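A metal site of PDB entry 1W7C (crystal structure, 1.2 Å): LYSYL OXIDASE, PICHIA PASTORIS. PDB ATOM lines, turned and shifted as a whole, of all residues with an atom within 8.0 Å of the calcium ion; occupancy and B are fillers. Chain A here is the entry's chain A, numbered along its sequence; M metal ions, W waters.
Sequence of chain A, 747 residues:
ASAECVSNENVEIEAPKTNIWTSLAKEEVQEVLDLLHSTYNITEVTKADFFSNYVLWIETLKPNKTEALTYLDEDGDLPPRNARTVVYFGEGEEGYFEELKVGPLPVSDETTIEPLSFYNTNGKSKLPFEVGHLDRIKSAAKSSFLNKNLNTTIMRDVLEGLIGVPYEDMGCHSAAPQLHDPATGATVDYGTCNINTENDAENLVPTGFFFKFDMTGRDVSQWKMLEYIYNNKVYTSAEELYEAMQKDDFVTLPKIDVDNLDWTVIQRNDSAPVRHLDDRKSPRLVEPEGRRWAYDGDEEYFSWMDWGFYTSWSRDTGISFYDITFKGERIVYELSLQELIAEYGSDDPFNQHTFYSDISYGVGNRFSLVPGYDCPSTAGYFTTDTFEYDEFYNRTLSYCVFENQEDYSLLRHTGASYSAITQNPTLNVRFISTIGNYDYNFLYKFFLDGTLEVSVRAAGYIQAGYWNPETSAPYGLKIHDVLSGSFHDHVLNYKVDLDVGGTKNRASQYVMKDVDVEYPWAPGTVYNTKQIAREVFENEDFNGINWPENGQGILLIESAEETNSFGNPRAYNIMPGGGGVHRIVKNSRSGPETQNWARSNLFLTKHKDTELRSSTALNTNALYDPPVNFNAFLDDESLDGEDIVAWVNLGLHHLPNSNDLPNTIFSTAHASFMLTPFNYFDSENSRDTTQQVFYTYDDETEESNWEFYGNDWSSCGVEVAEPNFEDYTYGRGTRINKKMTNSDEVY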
ATOM      1  N   GLU A 540      -0.326 -27.393  -5.637  1.00  0.00           N
ATOM      2  CA  GLU A 540       0.327 -26.102  -5.550  1.00  0.00           C
ATOM      3  C   GLU A 540       1.503 -26.111  -6.549  1.00  0.00           C
ATOM      4  O   GLU A 540       2.301 -27.047  -6.589  1.00  0.00           O
ATOM      5  CB  GLU A 540       0.850 -25.884  -4.131  1.00  0.00           C
ATOM      6  CG  GLU A 540      -0.219 -25.783  -3.097  1.00  0.00           C
ATOM      7  CD  GLU A 540       0.297 -25.751  -1.664  1.00  0.00           C
ATOM      8  OE1 GLU A 540       1.378 -26.341  -1.404  1.00  0.00           O
ATOM      9  OE2 GLU A 540      -0.395 -25.114  -0.812  1.00  0.00           O
ATOM     10  N   LEU A 604      -1.887 -20.119  -5.884  1.00  0.00           N
ATOM     11  CA  LEU A 604      -2.971 -20.865  -5.191  1.00  0.00           C
ATOM     12  C   LEU A 604      -2.360 -21.765  -4.153  1.00  0.00           C
ATOM     13  O   LEU A 604      -1.431 -22.531  -4.483  1.00  0.00           O
ATOM     14  CB  LEU A 604      -3.708 -21.711  -6.229  1.00  0.00           C
ATOM     15  CG  LEU A 604      -4.379 -20.918  -7.355  1.00  0.00           C
ATOM     16  CD1 LEU A 604      -4.935 -21.877  -8.406  1.00  0.00           C
ATOM     17  CD2 LEU A 604      -5.488 -20.024  -6.864  1.00  0.00           C
ATOM     18  N   THR A 605      -2.814 -21.679  -2.911  1.00  0.00           N
ATOM     19  CA  THR A 605      -2.316 -22.550  -1.859  1.00  0.00           C
ATOM     20  C   THR A 605      -3.438 -23.160  -1.062  1.00  0.00           C
ATOM     21  O   THR A 605      -4.584 -22.694  -1.074  1.00  0.00           O
ATOM     22  CB  THR A 605      -1.398 -21.799  -0.895  1.00  0.00           C
ATOM     23  OG1 THR A 605      -2.166 -20.814  -0.179  1.00  0.00           O
ATOM     24  CG2 THR A 605      -0.234 -21.084  -1.635  1.00  0.00           C
ATOM     25  N   LYS A 606      -3.089 -24.206  -0.312  1.00  0.00           N
ATOM     26  CA  LYS A 606      -3.995 -24.785   0.670  1.00  0.00           C
ATOM     27  C   LYS A 606      -4.061 -23.881   1.884  1.00  0.00           C
ATOM     28  O   LYS A 606      -3.040 -23.541   2.469  1.00  0.00           O
ATOM     29  CB  LYS A 606      -3.531 -26.214   1.013  1.00  0.00           C
ATOM     30  CG  LYS A 606      -4.253 -26.880   2.138  1.00  0.00           C
ATOM     31  CD  LYS A 606      -3.594 -28.250   2.459  1.00  0.00           C
ATOM     32  CE  LYS A 606      -4.170 -28.932   3.610  1.00  0.00           C
ATOM     33  NZ  LYS A 606      -3.563 -30.257   3.693  1.00  0.00           N
ATOM     34  N   HIS A 607      -5.255 -23.546   2.306  1.00  0.00           N
ATOM     35  CA  HIS A 607      -5.448 -22.680   3.459  1.00  0.00           C
ATOM     36  C   HIS A 607      -4.799 -23.275   4.687  1.00  0.00           C
ATOM     37  O   HIS A 607      -4.987 -24.456   4.972  1.00  0.00           O
ATOM     38  CB  HIS A 607      -6.913 -22.482   3.784  1.00  0.00           C
ATOM     39  CG  HIS A 607      -7.122 -21.561   4.949  1.00  0.00           C
ATOM     40  ND1 HIS A 607      -7.085 -22.013   6.249  1.00  0.00           N
ATOM     41  CD2 HIS A 607      -7.211 -20.222   5.005  1.00  0.00           C
ATOM     42  CE1 HIS A 607      -7.191 -20.965   7.063  1.00  0.00           C
ATOM     43  NE2 HIS A 607      -7.306 -19.869   6.327  1.00  0.00           N
ATOM     44  N   LYS A 608      -4.054 -22.465   5.439  1.00  0.00           N
ATOM     45  CA  LYS A 608      -3.534 -22.861   6.763  1.00  0.00           C
ATOM     46  C   LYS A 608      -3.561 -21.666   7.684  1.00  0.00           C
ATOM     47  O   LYS A 608      -3.227 -20.540   7.297  1.00  0.00           O
ATOM     48  CB  LYS A 608      -2.110 -23.373   6.653  1.00  0.00           C
ATOM     49  CG  LYS A 608      -1.957 -24.677   5.861  1.00  0.00           C
ATOM     50  CD  LYS A 608      -0.532 -25.177   5.759  1.00  0.00           C
ATOM     51  CE  LYS A 608      -0.491 -26.493   5.002  1.00  0.00           C
ATOM     52  NZ  LYS A 608       0.840 -27.074   4.813  1.00  0.00           N
ATOM     53  N   GLU A 611      -0.348 -20.034   7.777  1.00  0.00           N
ATOM     54  CA  GLU A 611      -0.030 -19.270   6.578  1.00  0.00           C
ATOM     55  C   GLU A 611      -1.044 -18.126   6.505  1.00  0.00           C
ATOM     56  O   GLU A 611      -1.825 -17.964   5.565  1.00  0.00           O
ATOM     57  CB  GLU A 611       0.052 -20.157   5.365  1.00  0.00           C
ATOM     58  CG  GLU A 611       1.120 -21.233   5.558  1.00  0.00           C
ATOM     59  CD  GLU A 611       1.311 -22.181   4.407  1.00  0.00           C
ATOM     60  OE1 GLU A 611       0.567 -22.114   3.404  1.00  0.00           O
ATOM     61  OE2 GLU A 611       2.235 -23.029   4.503  1.00  0.00           O
ATOM     62  N   PHE A 630       7.443 -16.479   1.780  1.00  0.00           N
ATOM     63  CA  PHE A 630       6.233 -16.918   1.103  1.00  0.00           C
ATOM     64  C   PHE A 630       6.429 -18.276   0.405  1.00  0.00           C
ATOM     65  O   PHE A 630       5.490 -19.040   0.275  1.00  0.00           O
ATOM     66  CB  PHE A 630       5.786 -15.863   0.119  1.00  0.00           C
ATOM     67  CG  PHE A 630       4.575 -16.241  -0.701  1.00  0.00           C
ATOM     68  CD1 PHE A 630       3.310 -16.121  -0.161  1.00  0.00           C
ATOM     69  CD2 PHE A 630       4.714 -16.739  -1.984  1.00  0.00           C
ATOM     70  CE1 PHE A 630       2.183 -16.441  -0.899  1.00  0.00           C
ATOM     71  CE2 PHE A 630       3.580 -17.075  -2.735  1.00  0.00           C
ATOM     72  CZ  PHE A 630       2.328 -16.951  -2.177  1.00  0.00           C
ATOM     73  N   ASN A 631       7.633 -18.535  -0.109  1.00  0.00           N
ATOM     74  CA  ASN A 631       7.853 -19.760  -0.832  1.00  0.00           C
ATOM     75  C   ASN A 631       7.669 -20.993   0.039  1.00  0.00           C
ATOM     76  O   ASN A 631       7.445 -22.074  -0.494  1.00  0.00           O
ATOM     77  CB  ASN A 631       9.260 -19.756  -1.444  1.00  0.00           C
ATOM     78  CG  ASN A 631       9.372 -18.880  -2.673  1.00  0.00           C
ATOM     79  OD1 ASN A 631       8.344 -18.424  -3.207  1.00  0.00           O
ATOM     80  ND2 ASN A 631      10.607 -18.604  -3.094  1.00  0.00           N
ATOM     81  N   ALA A 632       7.713 -20.854   1.369  1.00  0.00           N
ATOM     82  CA  ALA A 632       7.462 -21.969   2.263  1.00  0.00           C
ATOM     83  C   ALA A 632       6.036 -22.504   2.115  1.00  0.00           C
ATOM     84  O   ALA A 632       5.746 -23.652   2.456  1.00  0.00           O
ATOM     85  CB  ALA A 632       7.745 -21.586   3.711  1.00  0.00           C
ATOM     86  N   PHE A 633       5.103 -21.659   1.642  1.00  0.00           N
ATOM     87  CA  PHE A 633       3.720 -22.088   1.466  1.00  0.00           C
ATOM     88  C   PHE A 633       3.563 -23.084   0.308  1.00  0.00           C
ATOM     89  O   PHE A 633       2.574 -23.803   0.227  1.00  0.00           O
ATOM     90  CB  PHE A 633       2.792 -20.926   1.098  1.00  0.00           C
ATOM     91  CG  PHE A 633       2.683 -19.805   2.113  1.00  0.00           C
ATOM     92  CD1 PHE A 633       3.413 -19.787   3.300  1.00  0.00           C
ATOM     93  CD2 PHE A 633       1.814 -18.745   1.845  1.00  0.00           C
ATOM     94  CE1 PHE A 633       3.258 -18.676   4.188  1.00  0.00           C
ATOM     95  CE2 PHE A 633       1.684 -17.665   2.727  1.00  0.00           C
ATOM     96  CZ  PHE A 633       2.382 -17.666   3.919  1.00  0.00           C
ATOM     97  N   LEU A 634       4.533 -23.089  -0.611  1.00  0.00           N
ATOM     98  CA  LEU A 634       4.461 -23.790  -1.866  1.00  0.00           C
ATOM     99  C   LEU A 634       5.220 -25.085  -1.773  1.00  0.00           C
ATOM    100  O   LEU A 634       6.422 -25.156  -2.040  1.00  0.00           O
ATOM    101  CB  LEU A 634       5.049 -22.911  -2.986  1.00  0.00           C
ATOM    102  CG  LEU A 634       4.359 -21.576  -3.162  1.00  0.00           C
ATOM    103  CD1 LEU A 634       5.170 -20.639  -4.076  1.00  0.00           C
ATOM    104  CD2 LEU A 634       2.928 -21.761  -3.681  1.00  0.00           C
ATOM    105  N   ASP A 635       4.501 -26.122  -1.376  1.00  0.00           N
ATOM    106  CA  ASP A 635       5.105 -27.426  -1.081  1.00  0.00           C
ATOM    107  C   ASP A 635       4.282 -28.561  -1.694  1.00  0.00           C
ATOM    108  O   ASP A 635       4.217 -29.672  -1.189  1.00  0.00           O
ATOM    109  CB  ASP A 635       5.369 -27.599   0.423  1.00  0.00           C
ATOM    110  CG  ASP A 635       4.213 -27.196   1.299  1.00  0.00           C
ATOM    111  OD1 ASP A 635       4.430 -27.004   2.522  1.00  0.00           O
ATOM    112  OD2 ASP A 635       3.062 -27.064   0.845  1.00  0.00           O
ATOM    113  N   ASP A 636       3.745 -28.270  -2.886  1.00  0.00           N
ATOM    114  CA  ASP A 636       3.178 -29.277  -3.787  1.00  0.00           C
ATOM    115  C   ASP A 636       1.964 -29.983  -3.187  1.00  0.00           C
ATOM    116  O   ASP A 636       1.630 -31.089  -3.571  1.00  0.00           O
ATOM    117  CB  ASP A 636       4.236 -30.329  -4.164  1.00  0.00           C
ATOM    118  CG  ASP A 636       3.789 -31.247  -5.254  1.00  0.00           C
ATOM    119  OD1 ASP A 636       3.205 -30.711  -6.251  1.00  0.00           O
ATOM    120  OD2 ASP A 636       4.034 -32.513  -5.205  1.00  0.00           O
ATOM    121  N   GLU A 637       1.254 -29.297  -2.316  1.00  0.00           N
ATOM    122  CA  GLU A 637       0.104 -29.924  -1.685  1.00  0.00           C
ATOM    123  C   GLU A 637      -1.061 -30.014  -2.663  1.00  0.00           C
ATOM    124  O   GLU A 637      -1.206 -29.169  -3.535  1.00  0.00           O
ATOM    125  CB  GLU A 637      -0.311 -29.215  -0.410  1.00  0.00           C
ATOM    126  CG  GLU A 637       0.701 -29.395   0.719  1.00  0.00           C
ATOM    127  CD  GLU A 637       0.339 -28.617   1.967  1.00  0.00           C
ATOM    128  OE1 GLU A 637       0.095 -27.402   1.843  1.00  0.00           O
ATOM    129  OE2 GLU A 637       0.322 -29.204   3.072  1.00  0.00           O
ATOM    130  N   SER A 638      -1.833 -31.063  -2.546  1.00  0.00           N
ATOM    131  CA  SER A 638      -3.033 -31.205  -3.355  1.00  0.00           C
ATOM    132  C   SER A 638      -4.015 -30.071  -3.092  1.00  0.00           C
ATOM    133  O   SER A 638      -4.276 -29.697  -1.957  1.00  0.00           O
ATOM    134  CB  SER A 638      -3.737 -32.520  -3.069  1.00  0.00           C
ATOM    135  OG  SER A 638      -4.929 -32.628  -3.841  1.00  0.00           O
ATOM    136  N   LEU A 639      -4.563 -29.554  -4.184  1.00  0.00           N
ATOM    137  CA  LEU A 639      -5.620 -28.554  -4.131  1.00  0.00           C
ATOM    138  C   LEU A 639      -6.948 -29.146  -4.639  1.00  0.00           C
ATOM    139  O   LEU A 639      -7.912 -28.430  -4.850  1.00  0.00           O
ATOM    140  CB  LEU A 639      -5.253 -27.347  -5.002  1.00  0.00           C
ATOM    141  CG  LEU A 639      -3.982 -26.590  -4.595  1.00  0.00           C
ATOM    142  CD1 LEU A 639      -3.678 -25.519  -5.649  1.00  0.00           C
ATOM    143  CD2 LEU A 639      -4.064 -26.008  -3.217  1.00  0.00           C
HETATM  144 CA    CA M   1       1.233 -25.589   0.958  1.00  0.00          CA
HETATM  145  O   HOH W   1       2.326 -25.320   3.087  1.00  0.00           O
HETATM  146  O   HOH W   2      -0.329 -24.211   2.157  1.00  0.00           O
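The side-chain carboxylate of Glu 637 lies within salt-bridge range of the side-chain amino group of Lys 608 (2.8 Å).
The side-chain carboxylate (OE2) of Glu 540 sits close to the backbone NH (N) of Lys 606 (2.9 Å).
The backbone NH (N) of Asp 636 sits close to the side-chain carboxylate (OE1) of Glu 540, at 3.4 Å.
Of the 17 residues printed, 4 come within 4 Å of the calcium ion.
The nearest printed residue that does not touch the calcium ion is Lys 608 (4.1 Å).
The side-chain carboxylate (OE1) of Glu 637 is bound to the calcium ion (2.3 Å).
The backbone carbonyl oxygen (O) of Phe 633 binds the calcium ion, 2.3 Å away.
OD2 of Asp 635 binds the calcium ion.
Water W2 binds the calcium ion, 2.4 Å away.
The calcium ion is bound by water W1 (2.4 Å).
The calcium ion is bound by the side-chain carboxylate (OE2) of Glu 540 (2.5 Å).
OE1 of Glu 540 binds the calcium ion (2.5 Å).
The calcium ion has seven donor atoms within binding distance.
Water W1 lies within hydrogen-bond range of the side-chain carboxylate (OE2) of Glu 611 (2.7 Å), the side-chain carboxylate (OD1) of Asp 635 (2.8 Å) and the side-chain amino group (NZ) of Lys 608 (2.9 Å).
Water W2 bridges the side-chain carboxylate (OE1) of Glu 611 (2.6 Å) and the backbone carbonyl oxygen (O) of Lys 606 (2.8 Å).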
